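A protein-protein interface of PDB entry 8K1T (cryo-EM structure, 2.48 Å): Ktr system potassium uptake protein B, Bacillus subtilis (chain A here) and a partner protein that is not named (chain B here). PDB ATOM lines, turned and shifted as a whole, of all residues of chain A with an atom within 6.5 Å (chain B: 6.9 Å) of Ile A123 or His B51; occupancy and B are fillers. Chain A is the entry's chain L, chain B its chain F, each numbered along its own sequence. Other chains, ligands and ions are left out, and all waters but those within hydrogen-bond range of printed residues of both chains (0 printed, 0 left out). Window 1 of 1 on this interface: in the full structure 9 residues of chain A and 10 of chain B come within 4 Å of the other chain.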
ATOM      1  N   LEU A 108      -0.873  25.317  -0.698  1.00  0.00           N
ATOM      2  CA  LEU A 108       0.547  25.465  -0.992  1.00  0.00           C
ATOM      3  C   LEU A 108       1.417  25.045   0.185  1.00  0.00           C
ATOM      4  O   LEU A 108       2.435  24.376  -0.011  1.00  0.00           O
ATOM      5  CB  LEU A 108       0.855  26.910  -1.387  1.00  0.00           C
ATOM      6  CG  LEU A 108       2.310  27.203  -1.755  1.00  0.00           C
ATOM      7  CD1 LEU A 108       2.753  26.329  -2.916  1.00  0.00           C
ATOM      8  CD2 LEU A 108       2.493  28.672  -2.084  1.00  0.00           C
ATOM      9  N   ARG A 111       1.282  21.319   0.360  1.00  0.00           N
ATOM     10  CA  ARG A 111       2.007  20.730  -0.759  1.00  0.00           C
ATOM     11  C   ARG A 111       3.513  20.798  -0.554  1.00  0.00           C
ATOM     12  O   ARG A 111       4.242  19.931  -1.045  1.00  0.00           O
ATOM     13  CB  ARG A 111       1.611  21.427  -2.059  1.00  0.00           C
ATOM     14  CG  ARG A 111       1.719  20.553  -3.289  1.00  0.00           C
ATOM     15  CD  ARG A 111       1.111  21.222  -4.509  1.00  0.00           C
ATOM     16  NE  ARG A 111      -0.222  21.745  -4.237  1.00  0.00           N
ATOM     17  CZ  ARG A 111      -0.531  23.035  -4.221  1.00  0.00           C
ATOM     18  NH1 ARG A 111       0.371  23.965  -4.487  1.00  0.00           N
ATOM     19  NH2 ARG A 111      -1.777  23.400  -3.934  1.00  0.00           N
ATOM     20  N   MET A 112       3.996  21.817   0.157  1.00  0.00           N
ATOM     21  CA  MET A 112       5.421  21.897   0.460  1.00  0.00           C
ATOM     22  C   MET A 112       5.840  20.802   1.432  1.00  0.00           C
ATOM     23  O   MET A 112       6.964  20.292   1.354  1.00  0.00           O
ATOM     24  CB  MET A 112       5.760  23.277   1.020  1.00  0.00           C
ATOM     25  CG  MET A 112       5.638  24.398   0.002  1.00  0.00           C
ATOM     26  SD  MET A 112       5.834  26.036   0.726  1.00  0.00           S
ATOM     27  CE  MET A 112       7.512  25.936   1.339  1.00  0.00           C
ATOM     28  N   GLN A 115       6.389  17.668  -0.576  1.00  0.00           N
ATOM     29  CA  GLN A 115       7.661  17.740  -1.286  1.00  0.00           C
ATOM     30  C   GLN A 115       8.826  17.414  -0.359  1.00  0.00           C
ATOM     31  O   GLN A 115       9.753  16.693  -0.744  1.00  0.00           O
ATOM     32  CB  GLN A 115       7.831  19.128  -1.899  1.00  0.00           C
ATOM     33  CG  GLN A 115       9.063  19.284  -2.760  1.00  0.00           C
ATOM     34  CD  GLN A 115       9.543  20.717  -2.823  1.00  0.00           C
ATOM     35  OE1 GLN A 115       9.042  21.583  -2.108  1.00  0.00           O
ATOM     36  NE2 GLN A 115      10.524  20.974  -3.678  1.00  0.00           N
ATOM     37  N   GLN A 120      11.518  15.390  -2.784  1.00  0.00           N
ATOM     38  CA  GLN A 120      11.330  15.830  -4.160  1.00  0.00           C
ATOM     39  C   GLN A 120      11.970  17.199  -4.370  1.00  0.00           C
ATOM     40  O   GLN A 120      11.845  18.079  -3.515  1.00  0.00           O
ATOM     41  CB  GLN A 120       9.847  15.898  -4.502  1.00  0.00           C
ATOM     42  CG  GLN A 120       9.527  15.628  -5.961  1.00  0.00           C
ATOM     43  CD  GLN A 120       9.751  14.180  -6.349  1.00  0.00           C
ATOM     44  OE1 GLN A 120       9.865  13.303  -5.493  1.00  0.00           O
ATOM     45  NE2 GLN A 120       9.813  13.921  -7.650  1.00  0.00           N
ATOM     46  N   PRO A 121      12.679  17.403  -5.483  1.00  0.00           N
ATOM     47  CA  PRO A 121      13.272  18.725  -5.736  1.00  0.00           C
ATOM     48  C   PRO A 121      12.252  19.810  -6.031  1.00  0.00           C
ATOM     49  O   PRO A 121      12.503  20.974  -5.699  1.00  0.00           O
ATOM     50  CB  PRO A 121      14.184  18.473  -6.944  1.00  0.00           C
ATOM     51  CG  PRO A 121      13.571  17.305  -7.633  1.00  0.00           C
ATOM     52  CD  PRO A 121      13.003  16.438  -6.546  1.00  0.00           C
ATOM     53  N   THR A 122      11.113  19.473  -6.636  1.00  0.00           N
ATOM     54  CA  THR A 122      10.111  20.458  -7.019  1.00  0.00           C
ATOM     55  C   THR A 122       8.737  19.979  -6.572  1.00  0.00           C
ATOM     56  O   THR A 122       8.518  18.791  -6.324  1.00  0.00           O
ATOM     57  CB  THR A 122      10.114  20.712  -8.532  1.00  0.00           C
ATOM     58  OG1 THR A 122       9.863  19.483  -9.225  1.00  0.00           O
ATOM     59  CG2 THR A 122      11.451  21.282  -8.984  1.00  0.00           C
ATOM     60  N   ILE A 123       7.802  20.925  -6.475  1.00  0.00           N
ATOM     61  CA  ILE A 123       6.430  20.629  -6.079  1.00  0.00           C
ATOM     62  C   ILE A 123       5.555  20.272  -7.275  1.00  0.00           C
ATOM     63  O   ILE A 123       4.334  20.170  -7.135  1.00  0.00           O
ATOM     64  CB  ILE A 123       5.812  21.797  -5.295  1.00  0.00           C
ATOM     65  CG1 ILE A 123       6.022  23.112  -6.046  1.00  0.00           C
ATOM     66  CG2 ILE A 123       6.389  21.872  -3.896  1.00  0.00           C
ATOM     67  CD1 ILE A 123       5.418  24.309  -5.351  1.00  0.00           C
ATOM     68  N   GLY A 124       6.150  20.081  -8.449  1.00  0.00           N
ATOM     69  CA  GLY A 124       5.384  19.754  -9.632  1.00  0.00           C
ATOM     70  C   GLY A 124       4.813  18.353  -9.614  1.00  0.00           C
ATOM     71  O   GLY A 124       5.556  17.371  -9.703  1.00  0.00           O
ATOM     72  N   GLY A 125       3.494  18.250  -9.499  1.00  0.00           N
ATOM     73  CA  GLY A 125       2.834  16.956  -9.509  1.00  0.00           C
ATOM     74  C   GLY A 125       3.232  16.057  -8.361  1.00  0.00           C
ATOM     75  O   GLY A 125       3.459  14.859  -8.561  1.00  0.00           O
ATOM     76  N   VAL A 126       3.326  16.610  -7.155  1.00  0.00           N
ATOM     77  CA  VAL A 126       3.696  15.810  -5.996  1.00  0.00           C
ATOM     78  C   VAL A 126       2.456  15.219  -5.331  1.00  0.00           C
ATOM     79  O   VAL A 126       2.537  14.167  -4.689  1.00  0.00           O
ATOM     80  CB  VAL A 126       4.532  16.639  -5.000  1.00  0.00           C
ATOM     81  CG1 VAL A 126       3.672  17.663  -4.278  1.00  0.00           C
ATOM     82  CG2 VAL A 126       5.246  15.729  -4.016  1.00  0.00           C
ATOM     83  N   ILE A 127       1.305  15.879  -5.476  1.00  0.00           N
ATOM     84  CA  ILE A 127       0.058  15.305  -4.983  1.00  0.00           C
ATOM     85  C   ILE A 127      -0.364  14.126  -5.849  1.00  0.00           C
ATOM     86  O   ILE A 127      -0.868  13.115  -5.345  1.00  0.00           O
ATOM     87  CB  ILE A 127      -1.038  16.384  -4.910  1.00  0.00           C
ATOM     88  CG1 ILE A 127      -0.614  17.498  -3.955  1.00  0.00           C
ATOM     89  CG2 ILE A 127      -2.355  15.780  -4.454  1.00  0.00           C
ATOM     90  CD1 ILE A 127      -0.272  17.006  -2.568  1.00  0.00           C
ATOM     91  N   CYS B  22       2.766  40.707  -3.508  1.00  0.00           N
ATOM     92  CA  CYS B  22       3.146  39.596  -2.642  1.00  0.00           C
ATOM     93  C   CYS B  22       3.080  39.990  -1.172  1.00  0.00           C
ATOM     94  O   CYS B  22       2.523  39.262  -0.346  1.00  0.00           O
ATOM     95  CB  CYS B  22       4.551  39.110  -2.996  1.00  0.00           C
ATOM     96  SG  CYS B  22       4.628  37.964  -4.373  1.00  0.00           S
ATOM     97  N   GLU B  31      -1.991  32.354   0.760  1.00  0.00           N
ATOM     98  CA  GLU B  31      -0.887  31.551   0.243  1.00  0.00           C
ATOM     99  C   GLU B  31      -0.425  32.156  -1.075  1.00  0.00           C
ATOM    100  O   GLU B  31      -1.175  32.170  -2.056  1.00  0.00           O
ATOM    101  CB  GLU B  31      -1.318  30.099   0.064  1.00  0.00           C
ATOM    102  CG  GLU B  31      -1.593  29.367   1.365  1.00  0.00           C
ATOM    103  CD  GLU B  31      -2.045  27.934   1.149  1.00  0.00           C
ATOM    104  OE1 GLU B  31      -2.562  27.627   0.056  1.00  0.00           O
ATOM    105  OE2 GLU B  31      -1.879  27.112   2.076  1.00  0.00           O
ATOM    106  N   VAL B  32       0.805  32.656  -1.104  1.00  0.00           N
ATOM    107  CA  VAL B  32       1.353  33.338  -2.268  1.00  0.00           C
ATOM    108  C   VAL B  32       2.604  32.603  -2.721  1.00  0.00           C
ATOM    109  O   VAL B  32       3.499  32.334  -1.913  1.00  0.00           O
ATOM    110  CB  VAL B  32       1.672  34.813  -1.965  1.00  0.00           C
ATOM    111  CG1 VAL B  32       2.160  35.511  -3.217  1.00  0.00           C
ATOM    112  CG2 VAL B  32       0.453  35.510  -1.409  1.00  0.00           C
ATOM    113  N   LEU B  33       2.664  32.283  -4.007  1.00  0.00           N
ATOM    114  CA  LEU B  33       3.871  31.766  -4.632  1.00  0.00           C
ATOM    115  C   LEU B  33       4.539  32.902  -5.393  1.00  0.00           C
ATOM    116  O   LEU B  33       3.963  33.439  -6.343  1.00  0.00           O
ATOM    117  CB  LEU B  33       3.551  30.602  -5.569  1.00  0.00           C
ATOM    118  CG  LEU B  33       4.712  30.115  -6.435  1.00  0.00           C
ATOM    119  CD1 LEU B  33       5.821  29.544  -5.576  1.00  0.00           C
ATOM    120  CD2 LEU B  33       4.243  29.097  -7.450  1.00  0.00           C
ATOM    121  N   ALA B  34       5.744  33.269  -4.974  1.00  0.00           N
ATOM    122  CA  ALA B  34       6.497  34.344  -5.602  1.00  0.00           C
ATOM    123  C   ALA B  34       7.555  33.742  -6.513  1.00  0.00           C
ATOM    124  O   ALA B  34       8.438  33.017  -6.050  1.00  0.00           O
ATOM    125  CB  ALA B  34       7.139  35.245  -4.549  1.00  0.00           C
ATOM    126  N   VAL B  35       7.468  34.047  -7.803  1.00  0.00           N
ATOM    127  CA  VAL B  35       8.369  33.506  -8.812  1.00  0.00           C
ATOM    128  C   VAL B  35       9.121  34.664  -9.449  1.00  0.00           C
ATOM    129  O   VAL B  35       8.515  35.677  -9.814  1.00  0.00           O
ATOM    130  CB  VAL B  35       7.611  32.699  -9.880  1.00  0.00           C
ATOM    131  CG1 VAL B  35       8.585  32.004 -10.806  1.00  0.00           C
ATOM    132  CG2 VAL B  35       6.679  31.700  -9.227  1.00  0.00           C
ATOM    133  N   VAL B  42      14.325  36.937  -5.271  1.00  0.00           N
ATOM    134  CA  VAL B  42      13.656  35.834  -4.588  1.00  0.00           C
ATOM    135  C   VAL B  42      14.102  35.752  -3.134  1.00  0.00           C
ATOM    136  O   VAL B  42      13.294  35.479  -2.239  1.00  0.00           O
ATOM    137  CB  VAL B  42      13.911  34.516  -5.340  1.00  0.00           C
ATOM    138  CG1 VAL B  42      13.278  33.353  -4.605  1.00  0.00           C
ATOM    139  CG2 VAL B  42      13.371  34.609  -6.754  1.00  0.00           C
ATOM    140  N   TYR B  45      12.242  38.432  -1.024  1.00  0.00           N
ATOM    141  CA  TYR B  45      10.827  38.174  -0.797  1.00  0.00           C
ATOM    142  C   TYR B  45      10.556  36.776  -0.263  1.00  0.00           C
ATOM    143  O   TYR B  45       9.392  36.377  -0.172  1.00  0.00           O
ATOM    144  CB  TYR B  45      10.034  38.401  -2.084  1.00  0.00           C
ATOM    145  CG  TYR B  45       9.882  39.857  -2.441  1.00  0.00           C
ATOM    146  CD1 TYR B  45       8.856  40.618  -1.901  1.00  0.00           C
ATOM    147  CD2 TYR B  45      10.768  40.474  -3.309  1.00  0.00           C
ATOM    148  CE1 TYR B  45       8.718  41.950  -2.217  1.00  0.00           C
ATOM    149  CE2 TYR B  45      10.637  41.805  -3.633  1.00  0.00           C
ATOM    150  CZ  TYR B  45       9.610  42.539  -3.085  1.00  0.00           C
ATOM    151  OH  TYR B  45       9.478  43.869  -3.408  1.00  0.00           O
ATOM    152  N   ALA B  46      11.599  36.023   0.091  1.00  0.00           N
ATOM    153  CA  ALA B  46      11.390  34.687   0.635  1.00  0.00           C
ATOM    154  C   ALA B  46      10.622  34.731   1.949  1.00  0.00           C
ATOM    155  O   ALA B  46       9.912  33.777   2.288  1.00  0.00           O
ATOM    156  CB  ALA B  46      12.731  33.983   0.825  1.00  0.00           C
ATOM    157  N   TYR B  48       8.331  37.119   2.602  1.00  0.00           N
ATOM    158  CA  TYR B  48       7.044  37.749   2.345  1.00  0.00           C
ATOM    159  C   TYR B  48       6.144  36.895   1.467  1.00  0.00           C
ATOM    160  O   TYR B  48       5.157  37.399   0.925  1.00  0.00           O
ATOM    161  CB  TYR B  48       7.241  39.124   1.711  1.00  0.00           C
ATOM    162  CG  TYR B  48       7.936  40.111   2.611  1.00  0.00           C
ATOM    163  CD1 TYR B  48       7.255  40.732   3.648  1.00  0.00           C
ATOM    164  CD2 TYR B  48       9.273  40.427   2.424  1.00  0.00           C
ATOM    165  CE1 TYR B  48       7.885  41.634   4.474  1.00  0.00           C
ATOM    166  CE2 TYR B  48       9.912  41.329   3.245  1.00  0.00           C
ATOM    167  CZ  TYR B  48       9.214  41.931   4.268  1.00  0.00           C
ATOM    168  OH  TYR B  48       9.848  42.832   5.090  1.00  0.00           O
ATOM    169  N   ALA B  49       6.469  35.618   1.303  1.00  0.00           N
ATOM    170  CA  ALA B  49       5.661  34.712   0.508  1.00  0.00           C
ATOM    171  C   ALA B  49       5.648  33.347   1.173  1.00  0.00           C
ATOM    172  O   ALA B  49       6.587  32.970   1.877  1.00  0.00           O
ATOM    173  CB  ALA B  49       6.188  34.593  -0.928  1.00  0.00           C
ATOM    174  N   THR B  50       4.564  32.608   0.944  1.00  0.00           N
ATOM    175  CA  THR B  50       4.504  31.226   1.397  1.00  0.00           C
ATOM    176  C   THR B  50       5.581  30.384   0.729  1.00  0.00           C
ATOM    177  O   THR B  50       6.238  29.568   1.384  1.00  0.00           O
ATOM    178  CB  THR B  50       3.121  30.642   1.115  1.00  0.00           C
ATOM    179  OG1 THR B  50       2.132  31.386   1.833  1.00  0.00           O
ATOM    180  CG2 THR B  50       3.062  29.191   1.541  1.00  0.00           C
ATOM    181  N   HIS B  51       5.785  30.581  -0.569  1.00  0.00           N
ATOM    182  CA  HIS B  51       6.794  29.863  -1.327  1.00  0.00           C
ATOM    183  C   HIS B  51       7.431  30.822  -2.320  1.00  0.00           C
ATOM    184  O   HIS B  51       6.729  31.562  -3.012  1.00  0.00           O
ATOM    185  CB  HIS B  51       6.177  28.665  -2.054  1.00  0.00           C
ATOM    186  CG  HIS B  51       7.182  27.698  -2.591  1.00  0.00           C
ATOM    187  ND1 HIS B  51       6.843  26.671  -3.445  1.00  0.00           N
ATOM    188  CD2 HIS B  51       8.517  27.596  -2.391  1.00  0.00           C
ATOM    189  CE1 HIS B  51       7.926  25.980  -3.750  1.00  0.00           C
ATOM    190  NE2 HIS B  51       8.954  26.521  -3.124  1.00  0.00           N
ATOM    191  N   ALA B  52       8.759  30.817  -2.376  1.00  0.00           N
ATOM    192  CA  ALA B  52       9.499  31.663  -3.302  1.00  0.00           C
ATOM    193  C   ALA B  52      10.447  30.793  -4.108  1.00  0.00           C
ATOM    194  O   ALA B  52      11.230  30.028  -3.539  1.00  0.00           O
ATOM    195  CB  ALA B  52      10.271  32.758  -2.563  1.00  0.00           C
ATOM    196  N   VAL B  53      10.374  30.907  -5.430  1.00  0.00           N
ATOM    197  CA  VAL B  53      11.135  30.051  -6.330  1.00  0.00           C
ATOM    198  C   VAL B  53      11.876  30.919  -7.335  1.00  0.00           C
ATOM    199  O   VAL B  53      11.351  31.932  -7.807  1.00  0.00           O
ATOM    200  CB  VAL B  53      10.228  29.040  -7.063  1.00  0.00           C
ATOM    201  CG1 VAL B  53      11.071  28.040  -7.823  1.00  0.00           C
ATOM    202  CG2 VAL B  53       9.314  28.329  -6.085  1.00  0.00           C
ATOM    203  N   LEU B  64       5.575  23.952 -14.886  1.00  0.00           N
ATOM    204  CA  LEU B  64       4.904  22.767 -14.363  1.00  0.00           C
ATOM    205  C   LEU B  64       5.562  22.260 -13.086  1.00  0.00           C
ATOM    206  O   LEU B  64       4.887  21.661 -12.243  1.00  0.00           O
ATOM    207  CB  LEU B  64       4.881  21.666 -15.421  1.00  0.00           C
ATOM    208  CG  LEU B  64       3.974  21.921 -16.622  1.00  0.00           C
ATOM    209  CD1 LEU B  64       4.054  20.768 -17.609  1.00  0.00           C
ATOM    210  CD2 LEU B  64       2.543  22.138 -16.164  1.00  0.00           C
ATOM    211  N   SER B  65       6.866  22.488 -12.926  1.00  0.00           N
ATOM    212  CA  SER B  65       7.553  22.073 -11.709  1.00  0.00           C
ATOM    213  C   SER B  65       7.045  22.811 -10.479  1.00  0.00           C
ATOM    214  O   SER B  65       7.224  22.322  -9.360  1.00  0.00           O
ATOM    215  CB  SER B  65       9.059  22.287 -11.851  1.00  0.00           C
ATOM    216  OG  SER B  65       9.568  21.595 -12.976  1.00  0.00           O
ATOM    217  N   LEU B  66       6.424  23.972 -10.660  1.00  0.00           N
ATOM    218  CA  LEU B  66       5.874  24.749  -9.560  1.00  0.00           C
ATOM    219  C   LEU B  66       4.458  24.333  -9.194  1.00  0.00           C
ATOM    220  O   LEU B  66       3.916  24.842  -8.208  1.00  0.00           O
ATOM    221  CB  LEU B  66       5.883  26.239  -9.909  1.00  0.00           C
ATOM    222  CG  LEU B  66       7.208  26.802 -10.411  1.00  0.00           C
ATOM    223  CD1 LEU B  66       7.099  28.295 -10.647  1.00  0.00           C
ATOM    224  CD2 LEU B  66       8.304  26.490  -9.420  1.00  0.00           C
ATOM    225  N   GLY B  67       3.852  23.427  -9.951  1.00  0.00           N
ATOM    226  CA  GLY B  67       2.450  23.116  -9.728  1.00  0.00           C
ATOM    227  C   GLY B  67       1.551  24.304  -9.983  1.00  0.00           C
ATOM    228  O   GLY B  67       0.626  24.561  -9.203  1.00  0.00           O
ATOM    229  N   ILE B  68       1.806  25.040 -11.068  1.00  0.00           N
ATOM    230  CA  ILE B  68       1.076  26.270 -11.347  1.00  0.00           C
ATOM    231  C   ILE B  68      -0.401  26.028 -11.616  1.00  0.00           C
ATOM    232  O   ILE B  68      -1.199  26.965 -11.512  1.00  0.00           O
ATOM    233  CB  ILE B  68       1.728  27.007 -12.535  1.00  0.00           C
ATOM    234  CG1 ILE B  68       1.415  28.502 -12.484  1.00  0.00           C
ATOM    235  CG2 ILE B  68       1.272  26.413 -13.851  1.00  0.00           C
ATOM    236  CD1 ILE B  68       2.102  29.225 -11.355  1.00  0.00           C
ATOM    237  N   ASN B  70      -2.385  24.577  -9.726  1.00  0.00           N
ATOM    238  CA  ASN B  70      -3.087  24.588  -8.453  1.00  0.00           C
ATOM    239  C   ASN B  70      -3.515  25.983  -8.022  1.00  0.00           C
ATOM    240  O   ASN B  70      -4.143  26.123  -6.969  1.00  0.00           O
ATOM    241  CB  ASN B  70      -2.207  23.962  -7.369  1.00  0.00           C
ATOM    242  CG  ASN B  70      -1.815  22.537  -7.692  1.00  0.00           C
ATOM    243  OD1 ASN B  70      -0.633  22.216  -7.806  1.00  0.00           O
ATOM    244  ND2 ASN B  70      -2.808  21.672  -7.846  1.00  0.00           N
ATOM    245  N   PHE B  71      -3.201  27.011  -8.804  1.00  0.00           N
ATOM    246  CA  PHE B  71      -3.513  28.391  -8.460  1.00  0.00           C
ATOM    247  C   PHE B  71      -4.662  28.887  -9.324  1.00  0.00           C
ATOM    248  O   PHE B  71      -4.634  28.734 -10.548  1.00  0.00           O
ATOM    249  CB  PHE B  71      -2.289  29.289  -8.641  1.00  0.00           C
ATOM    250  CG  PHE B  71      -1.118  28.883  -7.804  1.00  0.00           C
ATOM    251  CD1 PHE B  71      -1.001  29.318  -6.499  1.00  0.00           C
ATOM    252  CD2 PHE B  71      -0.136  28.059  -8.316  1.00  0.00           C
ATOM    253  CE1 PHE B  71       0.071  28.944  -5.723  1.00  0.00           C
ATOM    254  CE2 PHE B  71       0.939  27.680  -7.545  1.00  0.00           C
ATOM    255  CZ  PHE B  71       1.042  28.123  -6.247  1.00  0.00           C
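Of chain B, only His B51, Ser B65 and Leu B66 come within 4 Å of Ile A123. Of the printed residues of chain B, Gly A124 touches Leu B64 (3.3 Å), Ser B65 (2.6 Å) and Gly B67 (3.99 Å). Of chain A, only Leu A108, Met A112 and Ile A123 come within 4 Å of His B51. Of the printed residues of chain A, Leu B64 touches Gly A124. Of the printed residues of chain A, Ser B65 touches Thr A122, Ile A123 and Gly A124. Of the printed residues of chain A, Leu B66 touches Ile A123. The nearest residue of chain B that does not touch Ile A123 is Gly B67 (4.3 Å). The nearest residue of chain A that does not touch His B51 is Gln A115 (4.8 Å). The nearest printed residue of chain A that does not touch Gly B67 is Ile A123 (4.3 Å).
The backbone carbonyl oxygen (O) of Ser B65 sits at hydrogen-bond distance from the backbone NH (N) of Ile A123, 3.3 Å away. The backbone NH (N) of Leu A108 is in hydrogen-bond range of the side-chain carboxylate (OE1) of Glu B31, 3.0 Å away. O of Ser B65 sits at hydrogen-bond distance from N of Gly A124, at 2.6 Å. O of Thr B50 sits close to SD of Met A112.
Among the printed residues, pairs that only touch across the chains: Gly A124 with Leu B64 (3.3 Å), Ile A123 with Leu B66 (3.3 Å), Ile A123 with His B51 (3.4 Å), Thr A122 with Ser B65 (3.4 Å), Arg A111 with Asn B70 (3.5 Å), Leu A108 with His B51 (3.7 Å), Leu A108 with Thr B50 (3.7 Å), Leu A108 with Val B32 (3.8 Å), Met A112 with His B51 (3.8 Å) and Gly A124 with Gly B67 (3.99 Å).
Hydrophobic or aromatic side chains of chain B that line the printed part of chain A: His B51. Hydrophobic or aromatic side chains of chain A within 4 Å of the printed part of chain B: Leu A108, Met A112 and Ile A123. Among the printed residues, 14 pairs touch across the chains. Among the printed residues, no Asp or Glu carboxylate lies within 4 Å of a Lys or Arg side-chain nitrogen of the other chain.
O of Gly B67 sits close to OD1 of Asn B70 (3.0 Å). O of Val B32 sits at hydrogen-bond distance from N of His B51 (3.2 Å). N of Thr A122 sits close to NE2 of Gln A115 (3.4 Å). The backbone carbonyl oxygen (O) of Val B32 is in hydrogen-bond range of the backbone NH (N) of Thr B50, 3.1 Å away. O of His B51 sits at hydrogen-bond distance from N of Ala B34, at 2.8 Å.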
